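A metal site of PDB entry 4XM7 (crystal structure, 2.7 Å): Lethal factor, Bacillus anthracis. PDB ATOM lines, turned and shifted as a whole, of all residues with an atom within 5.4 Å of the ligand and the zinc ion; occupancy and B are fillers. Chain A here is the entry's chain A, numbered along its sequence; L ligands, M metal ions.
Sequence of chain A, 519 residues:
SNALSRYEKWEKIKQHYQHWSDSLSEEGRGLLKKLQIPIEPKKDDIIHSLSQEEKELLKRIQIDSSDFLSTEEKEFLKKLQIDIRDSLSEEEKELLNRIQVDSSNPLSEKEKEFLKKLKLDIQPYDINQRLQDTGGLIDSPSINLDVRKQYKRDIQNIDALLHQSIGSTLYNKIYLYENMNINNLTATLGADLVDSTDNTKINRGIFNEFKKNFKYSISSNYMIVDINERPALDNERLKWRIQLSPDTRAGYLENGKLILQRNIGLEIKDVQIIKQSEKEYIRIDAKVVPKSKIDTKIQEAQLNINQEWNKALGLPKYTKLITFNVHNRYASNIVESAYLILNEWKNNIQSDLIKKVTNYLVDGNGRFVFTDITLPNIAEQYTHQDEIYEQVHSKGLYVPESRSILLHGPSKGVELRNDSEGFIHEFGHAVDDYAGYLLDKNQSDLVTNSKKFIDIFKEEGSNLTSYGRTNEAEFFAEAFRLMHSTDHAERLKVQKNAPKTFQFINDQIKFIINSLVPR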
ATOM      1  N   ASP A  67      29.956  23.965  33.848  1.00  0.00           N
ATOM      2  CA  ASP A  67      29.141  23.590  32.697  1.00  0.00           C
ATOM      3  C   ASP A  67      29.675  24.152  31.381  1.00  0.00           C
ATOM      4  O   ASP A  67      29.290  23.687  30.306  1.00  0.00           O
ATOM      5  CB  ASP A  67      27.693  24.072  32.920  1.00  0.00           C
ATOM      6  CG  ASP A  67      27.609  25.556  33.252  1.00  0.00           C
ATOM      7  OD1 ASP A  67      28.341  26.362  32.640  1.00  0.00           O
ATOM      8  OD2 ASP A  67      26.792  25.921  34.117  1.00  0.00           O
ATOM      9  N   VAL A 392      30.545  30.541  25.880  1.00  0.00           N
ATOM     10  CA  VAL A 392      30.182  29.282  26.527  1.00  0.00           C
ATOM     11  C   VAL A 392      30.223  28.134  25.544  1.00  0.00           C
ATOM     12  O   VAL A 392      29.691  28.230  24.439  1.00  0.00           O
ATOM     13  CB  VAL A 392      28.760  29.356  27.145  1.00  0.00           C
ATOM     14  CG1 VAL A 392      28.351  28.004  27.713  1.00  0.00           C
ATOM     15  CG2 VAL A 392      28.694  30.436  28.219  1.00  0.00           C
ATOM     16  N   SER A 394      28.852  24.252  25.502  1.00  0.00           N
ATOM     17  CA  SER A 394      28.007  23.268  26.153  1.00  0.00           C
ATOM     18  C   SER A 394      27.253  22.558  25.037  1.00  0.00           C
ATOM     19  O   SER A 394      27.388  22.936  23.880  1.00  0.00           O
ATOM     20  CB  SER A 394      27.064  23.924  27.153  1.00  0.00           C
ATOM     21  OG  SER A 394      26.352  24.999  26.552  1.00  0.00           O
ATOM     22  N   LYS A 395      26.475  21.540  25.376  1.00  0.00           N
ATOM     23  CA  LYS A 395      25.755  20.811  24.336  1.00  0.00           C
ATOM     24  C   LYS A 395      24.697  21.713  23.698  1.00  0.00           C
ATOM     25  O   LYS A 395      24.402  21.579  22.510  1.00  0.00           O
ATOM     26  CB  LYS A 395      25.112  19.545  24.898  1.00  0.00           C
ATOM     27  CG  LYS A 395      24.299  18.773  23.873  1.00  0.00           C
ATOM     28  CD  LYS A 395      24.312  17.280  24.138  1.00  0.00           C
ATOM     29  CE  LYS A 395      23.657  16.524  22.999  1.00  0.00           C
ATOM     30  NZ  LYS A 395      24.420  16.676  21.725  1.00  0.00           N
ATOM     31  N   GLY A 396      24.147  22.637  24.479  1.00  0.00           N
ATOM     32  CA  GLY A 396      23.113  23.525  23.991  1.00  0.00           C
ATOM     33  C   GLY A 396      23.064  24.854  24.690  1.00  0.00           C
ATOM     34  O   GLY A 396      23.645  25.046  25.758  1.00  0.00           O
ATOM     35  N   LEU A 397      22.330  25.795  24.090  1.00  0.00           N
ATOM     36  CA  LEU A 397      22.244  27.157  24.611  1.00  0.00           C
ATOM     37  C   LEU A 397      21.029  27.870  24.037  1.00  0.00           C
ATOM     38  O   LEU A 397      20.609  27.597  22.911  1.00  0.00           O
ATOM     39  CB  LEU A 397      23.526  27.926  24.269  1.00  0.00           C
ATOM     40  CG  LEU A 397      24.064  28.934  25.272  1.00  0.00           C
ATOM     41  CD1 LEU A 397      24.434  28.245  26.574  1.00  0.00           C
ATOM     42  CD2 LEU A 397      25.270  29.673  24.691  1.00  0.00           C
ATOM     43  N   TYR A 398      20.457  28.790  24.817  1.00  0.00           N
ATOM     44  CA  TYR A 398      19.512  29.743  24.259  1.00  0.00           C
ATOM     45  C   TYR A 398      20.072  31.142  24.412  1.00  0.00           C
ATOM     46  O   TYR A 398      20.448  31.561  25.513  1.00  0.00           O
ATOM     47  CB  TYR A 398      18.138  29.652  24.933  1.00  0.00           C
ATOM     48  CG  TYR A 398      17.224  30.776  24.495  1.00  0.00           C
ATOM     49  CD1 TYR A 398      16.673  30.782  23.225  1.00  0.00           C
ATOM     50  CD2 TYR A 398      16.936  31.838  25.343  1.00  0.00           C
ATOM     51  CE1 TYR A 398      15.843  31.819  22.803  1.00  0.00           C
ATOM     52  CE2 TYR A 398      16.110  32.879  24.929  1.00  0.00           C
ATOM     53  CZ  TYR A 398      15.573  32.857  23.666  1.00  0.00           C
ATOM     54  OH  TYR A 398      14.755  33.876  23.246  1.00  0.00           O
ATOM     55  N   LEU A 407      22.373  24.003  19.269  1.00  0.00           N
ATOM     56  CA  LEU A 407      22.493  22.615  19.699  1.00  0.00           C
ATOM     57  C   LEU A 407      23.688  21.937  19.061  1.00  0.00           C
ATOM     58  O   LEU A 407      23.733  21.734  17.847  1.00  0.00           O
ATOM     59  CB  LEU A 407      21.207  21.846  19.374  1.00  0.00           C
ATOM     60  CG  LEU A 407      20.987  20.640  20.290  1.00  0.00           C
ATOM     61  CD1 LEU A 407      20.685  21.130  21.687  1.00  0.00           C
ATOM     62  CD2 LEU A 407      19.858  19.762  19.779  1.00  0.00           C
ATOM     63  N   LYS A 412      28.391  15.627  24.901  1.00  0.00           N
ATOM     64  CA  LYS A 412      27.507  14.928  25.830  1.00  0.00           C
ATOM     65  C   LYS A 412      26.842  15.903  26.794  1.00  0.00           C
ATOM     66  O   LYS A 412      27.425  16.913  27.167  1.00  0.00           O
ATOM     67  CB  LYS A 412      28.292  13.872  26.616  1.00  0.00           C
ATOM     68  CG  LYS A 412      27.446  13.033  27.558  1.00  0.00           C
ATOM     69  CD  LYS A 412      28.287  11.971  28.274  1.00  0.00           C
ATOM     70  CE  LYS A 412      27.438  11.149  29.233  1.00  0.00           C
ATOM     71  NZ  LYS A 412      28.236  10.102  29.949  1.00  0.00           N
ATOM     72  N   GLY A 413      25.624  15.585  27.205  1.00  0.00           N
ATOM     73  CA  GLY A 413      24.887  16.466  28.102  1.00  0.00           C
ATOM     74  C   GLY A 413      25.122  16.188  29.571  1.00  0.00           C
ATOM     75  O   GLY A 413      25.475  15.074  29.958  1.00  0.00           O
ATOM     76  N   VAL A 414      24.939  17.222  30.385  1.00  0.00           N
ATOM     77  CA  VAL A 414      25.024  17.073  31.836  1.00  0.00           C
ATOM     78  C   VAL A 414      23.814  16.281  32.311  1.00  0.00           C
ATOM     79  O   VAL A 414      22.720  16.822  32.467  1.00  0.00           O
ATOM     80  CB  VAL A 414      25.080  18.448  32.549  1.00  0.00           C
ATOM     81  CG1 VAL A 414      24.908  18.288  34.062  1.00  0.00           C
ATOM     82  CG2 VAL A 414      26.382  19.153  32.228  1.00  0.00           C
ATOM     83  N   LEU A 416      21.599  13.952  30.943  1.00  0.00           N
ATOM     84  CA  LEU A 416      20.359  14.102  30.190  1.00  0.00           C
ATOM     85  C   LEU A 416      20.249  13.044  29.114  1.00  0.00           C
ATOM     86  O   LEU A 416      21.223  12.732  28.427  1.00  0.00           O
ATOM     87  CB  LEU A 416      20.266  15.500  29.576  1.00  0.00           C
ATOM     88  CG  LEU A 416      18.864  16.111  29.635  1.00  0.00           C
ATOM     89  CD1 LEU A 416      18.487  16.358  31.085  1.00  0.00           C
ATOM     90  CD2 LEU A 416      18.771  17.390  28.827  1.00  0.00           C
ATOM     91  N   ASN A 418      18.610  12.475  25.968  1.00  0.00           N
ATOM     92  CA  ASN A 418      18.716  12.596  24.527  1.00  0.00           C
ATOM     93  C   ASN A 418      18.712  14.065  24.138  1.00  0.00           C
ATOM     94  O   ASN A 418      18.408  14.936  24.951  1.00  0.00           O
ATOM     95  CB  ASN A 418      17.683  11.828  23.695  1.00  0.00           C
ATOM     96  CG  ASN A 418      16.266  12.081  24.155  1.00  0.00           C
ATOM     97  OD1 ASN A 418      15.836  13.225  24.301  1.00  0.00           O
ATOM     98  ND2 ASN A 418      15.527  11.004  24.408  1.00  0.00           N
ATOM     99  N   ASP A 419      19.067  14.336  22.884  1.00  0.00           N
ATOM    100  CA  ASP A 419      19.086  15.687  22.349  1.00  0.00           C
ATOM    101  C   ASP A 419      17.692  16.309  22.376  1.00  0.00           C
ATOM    102  O   ASP A 419      17.543  17.503  22.634  1.00  0.00           O
ATOM    103  CB  ASP A 419      19.621  15.700  20.909  1.00  0.00           C
ATOM    104  CG  ASP A 419      21.013  15.114  20.807  1.00  0.00           C
ATOM    105  OD1 ASP A 419      21.378  14.292  21.685  1.00  0.00           O
ATOM    106  OD2 ASP A 419      21.737  15.473  19.860  1.00  0.00           O
ATOM    107  N   GLU A 421      15.175  15.975  24.430  1.00  0.00           N
ATOM    108  CA  GLU A 421      14.785  16.499  25.731  1.00  0.00           C
ATOM    109  C   GLU A 421      15.515  17.806  26.018  1.00  0.00           C
ATOM    110  O   GLU A 421      14.972  18.726  26.618  1.00  0.00           O
ATOM    111  CB  GLU A 421      15.060  15.491  26.844  1.00  0.00           C
ATOM    112  CG  GLU A 421      14.070  14.328  26.882  1.00  0.00           C
ATOM    113  CD  GLU A 421      14.124  13.552  28.188  1.00  0.00           C
ATOM    114  OE1 GLU A 421      15.214  13.454  28.780  1.00  0.00           O
ATOM    115  OE2 GLU A 421      13.078  13.032  28.616  1.00  0.00           O
ATOM    116  N   GLY A 422      16.762  17.889  25.548  1.00  0.00           N
ATOM    117  CA  GLY A 422      17.548  19.092  25.739  1.00  0.00           C
ATOM    118  C   GLY A 422      17.074  20.264  24.914  1.00  0.00           C
ATOM    119  O   GLY A 422      17.195  21.417  25.333  1.00  0.00           O
ATOM    120  N   PHE A 423      16.519  19.988  23.731  1.00  0.00           N
ATOM    121  CA  PHE A 423      15.980  21.041  22.883  1.00  0.00           C
ATOM    122  C   PHE A 423      14.742  21.657  23.522  1.00  0.00           C
ATOM    123  O   PHE A 423      14.553  22.878  23.475  1.00  0.00           O
ATOM    124  CB  PHE A 423      15.627  20.503  21.493  1.00  0.00           C
ATOM    125  CG  PHE A 423      15.132  21.570  20.547  1.00  0.00           C
ATOM    126  CD1 PHE A 423      16.021  22.338  19.822  1.00  0.00           C
ATOM    127  CD2 PHE A 423      13.767  21.789  20.392  1.00  0.00           C
ATOM    128  CE1 PHE A 423      15.565  23.314  18.962  1.00  0.00           C
ATOM    129  CE2 PHE A 423      13.309  22.774  19.528  1.00  0.00           C
ATOM    130  CZ  PHE A 423      14.212  23.537  18.810  1.00  0.00           C
ATOM    131  N   HIS A 425      14.148  21.780  26.654  1.00  0.00           N
ATOM    132  CA  HIS A 425      14.701  22.606  27.712  1.00  0.00           C
ATOM    133  C   HIS A 425      15.073  23.988  27.182  1.00  0.00           C
ATOM    134  O   HIS A 425      14.744  25.006  27.795  1.00  0.00           O
ATOM    135  CB  HIS A 425      15.921  21.917  28.320  1.00  0.00           C
ATOM    136  CG  HIS A 425      16.730  22.789  29.241  1.00  0.00           C
ATOM    137  ND1 HIS A 425      16.771  22.584  30.595  1.00  0.00           N
ATOM    138  CD2 HIS A 425      17.543  23.833  28.981  1.00  0.00           C
ATOM    139  CE1 HIS A 425      17.577  23.485  31.145  1.00  0.00           C
ATOM    140  NE2 HIS A 425      18.045  24.253  30.192  1.00  0.00           N
ATOM    141  N   GLU A 426      15.752  24.023  26.037  1.00  0.00           N
ATOM    142  CA  GLU A 426      16.152  25.279  25.422  1.00  0.00           C
ATOM    143  C   GLU A 426      14.932  26.088  24.984  1.00  0.00           C
ATOM    144  O   GLU A 426      14.897  27.304  25.133  1.00  0.00           O
ATOM    145  CB  GLU A 426      17.074  25.046  24.233  1.00  0.00           C
ATOM    146  CG  GLU A 426      18.348  24.273  24.571  1.00  0.00           C
ATOM    147  CD  GLU A 426      19.289  25.040  25.468  1.00  0.00           C
ATOM    148  OE1 GLU A 426      20.297  24.451  25.899  1.00  0.00           O
ATOM    149  OE2 GLU A 426      19.036  26.231  25.739  1.00  0.00           O
ATOM    150  N   HIS A 429      13.533  28.122  27.606  1.00  0.00           N
ATOM    151  CA  HIS A 429      14.169  29.424  27.782  1.00  0.00           C
ATOM    152  C   HIS A 429      13.483  30.489  26.948  1.00  0.00           C
ATOM    153  O   HIS A 429      13.238  31.602  27.407  1.00  0.00           O
ATOM    154  CB  HIS A 429      15.640  29.349  27.394  1.00  0.00           C
ATOM    155  CG  HIS A 429      16.530  28.856  28.488  1.00  0.00           C
ATOM    156  ND1 HIS A 429      16.446  29.324  29.786  1.00  0.00           N
ATOM    157  CD2 HIS A 429      17.538  27.956  28.480  1.00  0.00           C
ATOM    158  CE1 HIS A 429      17.362  28.730  30.523  1.00  0.00           C
ATOM    159  NE2 HIS A 429      18.041  27.892  29.763  1.00  0.00           N
ATOM    160  N   TYR A 467      20.824  20.076  38.344  1.00  0.00           N
ATOM    161  CA  TYR A 467      21.292  21.215  37.563  1.00  0.00           C
ATOM    162  C   TYR A 467      20.305  22.377  37.617  1.00  0.00           C
ATOM    163  O   TYR A 467      20.694  23.529  37.438  1.00  0.00           O
ATOM    164  CB  TYR A 467      21.522  20.829  36.101  1.00  0.00           C
ATOM    165  CG  TYR A 467      22.070  21.976  35.304  1.00  0.00           C
ATOM    166  CD1 TYR A 467      23.329  22.496  35.591  1.00  0.00           C
ATOM    167  CD2 TYR A 467      21.331  22.585  34.302  1.00  0.00           C
ATOM    168  CE1 TYR A 467      23.839  23.572  34.880  1.00  0.00           C
ATOM    169  CE2 TYR A 467      21.828  23.657  33.586  1.00  0.00           C
ATOM    170  CZ  TYR A 467      23.092  24.150  33.884  1.00  0.00           C
ATOM    171  OH  TYR A 467      23.596  25.207  33.184  1.00  0.00           O
ATOM    172  N   GLU A 474      17.597  28.627  34.736  1.00  0.00           N
ATOM    173  CA  GLU A 474      17.806  27.197  34.513  1.00  0.00           C
ATOM    174  C   GLU A 474      16.701  26.375  35.171  1.00  0.00           C
ATOM    175  O   GLU A 474      16.252  25.381  34.610  1.00  0.00           O
ATOM    176  CB  GLU A 474      19.172  26.759  35.058  1.00  0.00           C
ATOM    177  CG  GLU A 474      20.349  27.658  34.678  1.00  0.00           C
ATOM    178  CD  GLU A 474      20.684  27.648  33.184  1.00  0.00           C
ATOM    179  OE1 GLU A 474      19.914  27.054  32.402  1.00  0.00           O
ATOM    180  OE2 GLU A 474      21.718  28.228  32.804  1.00  0.00           O
ATOM    181  N   ALA A 477      13.632  26.230  33.210  1.00  0.00           N
ATOM    182  CA  ALA A 477      13.839  25.454  31.989  1.00  0.00           C
ATOM    183  C   ALA A 477      13.774  23.945  32.249  1.00  0.00           C
ATOM    184  O   ALA A 477      13.157  23.212  31.487  1.00  0.00           O
ATOM    185  CB  ALA A 477      15.178  25.817  31.359  1.00  0.00           C
ATOM    186  N   GLU A 478      14.397  23.499  33.335  1.00  0.00           N
ATOM    187  CA  GLU A 478      14.352  22.095  33.716  1.00  0.00           C
ATOM    188  C   GLU A 478      12.944  21.676  34.094  1.00  0.00           C
ATOM    189  O   GLU A 478      12.499  20.576  33.760  1.00  0.00           O
ATOM    190  CB  GLU A 478      15.309  21.809  34.862  1.00  0.00           C
ATOM    191  CG  GLU A 478      16.766  21.687  34.442  1.00  0.00           C
ATOM    192  CD  GLU A 478      17.029  20.465  33.585  1.00  0.00           C
ATOM    193  OE1 GLU A 478      17.564  19.469  34.109  1.00  0.00           O
ATOM    194  OE2 GLU A 478      16.703  20.503  32.378  1.00  0.00           O
HETATM  195  C1  LIG L   1      22.919  23.861  28.859  1.00  0.00           C
HETATM  196  C2  LIG L   1      21.718  24.717  29.119  1.00  0.00           C
HETATM  197  C3  LIG L   1      21.709  16.697  26.849  1.00  0.00           C
HETATM  198  O1  LIG L   1      19.968  26.003  28.361  1.00  0.00           O
HETATM  199  N1  LIG L   1      22.681  22.473  29.201  1.00  0.00           N
HETATM  200  C4  LIG L   1      24.274  25.815  29.683  1.00  0.00           C
HETATM  201  C5  LIG L   1      25.344  23.550  29.440  1.00  0.00           C
HETATM  202  C6  LIG L   1      22.451  20.800  27.298  1.00  0.00           C
HETATM  203  C7  LIG L   1      22.310  19.426  27.076  1.00  0.00           C
HETATM  204  C8  LIG L   1      21.503  18.977  26.039  1.00  0.00           C
HETATM  205  C9  LIG L   1      20.836  19.880  25.224  1.00  0.00           C
HETATM  206  C10 LIG L   1      20.979  21.244  25.450  1.00  0.00           C
HETATM  207  C11 LIG L   1      21.785  21.702  26.483  1.00  0.00           C
HETATM  208  O2  LIG L   1      21.365  17.630  25.827  1.00  0.00           O
HETATM  209  C12 LIG L   1      20.822  21.143  29.792  1.00  0.00           C
HETATM  210  C13 LIG L   1      21.721  22.265  30.280  1.00  0.00           C
HETATM  211  C14 LIG L   1      24.064  24.310  29.768  1.00  0.00           C
HETATM  212  N2  LIG L   1      21.042  25.250  28.087  1.00  0.00           N
HETATM  213  O3  LIG L   1      21.211  25.004  30.453  1.00  0.00           O
HETATM  214  S1  LIG L   1      23.372  21.318  28.489  1.00  0.00           S
HETATM  215  O4  LIG L   1      23.608  20.253  29.419  1.00  0.00           O
HETATM  216  O5  LIG L   1      24.621  21.767  27.954  1.00  0.00           O
HETATM  217  F1  LIG L   1      20.057  19.428  24.225  1.00  0.00           F
HETATM  218  C15 LIG L   1      20.466  20.200  30.943  1.00  0.00           C
HETATM  219  C16 LIG L   1      19.564  21.692  29.122  1.00  0.00           C
HETATM  220 ZN    ZN M   1      19.534  26.215  30.390  1.00  0.00          ZN
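Residues that only touch the ligand: Ser 394 (2.9 Å), Gly 422 (2.9 Å), Leu 407 (3.1 Å), Leu 416 (3.3 Å), Gly 413 (3.4 Å), Tyr 467 (3.5 Å), Asp 419 (3.5 Å), Phe 423 (3.6 Å) and Leu 397 (3.9 Å). Of the 24 residues printed, 16 come within 4 Å of the ligand. Along chain A the residues within 4 Å of the ligand span positions 394 to 474.
The zinc ion is bound by O3 of the ligand (2.1 Å), O1 of the ligand (2.1 Å), OE1 of Glu 474 (2.2 Å), NE2 of His 429 (2.3 Å) and NE2 of His 425 (2.5 Å).
A nitrogen (N2) of the ligand is in hydrogen-bond range of the side-chain carboxylate of Glu 426 (2.4 Å). The backbone NH (N) of Lys 395 lies within hydrogen-bond range of an oxygen (O5) of the ligand. A nitrogen (N2) of the ligand lies close to the backbone carbonyl oxygen of Gly 396, at 3.5 Å. An oxygen (O4) of the ligand sits at hydrogen-bond distance from the backbone NH of Val 414, at 3.4 Å.
OE1 of Glu 426 sits at hydrogen-bond distance from N of Leu 397 (3.0 Å). N of Tyr 398 is in hydrogen-bond range of OE2 of Glu 426 (3.1 Å). ND1 of His 425 is in hydrogen-bond range of OE2 of Glu 478, at 2.7 Å. The backbone carbonyl oxygen of Gly 396 is in hydrogen-bond range of the side-chain hydroxyl of Ser 394 (2.8 Å). The side-chain amino group of Lys 395 lies within salt-bridge range of the side-chain carboxylate of Asp 419. OD2 of Asp 67 lies within hydrogen-bond range of OH of Tyr 467 (3.4 Å).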
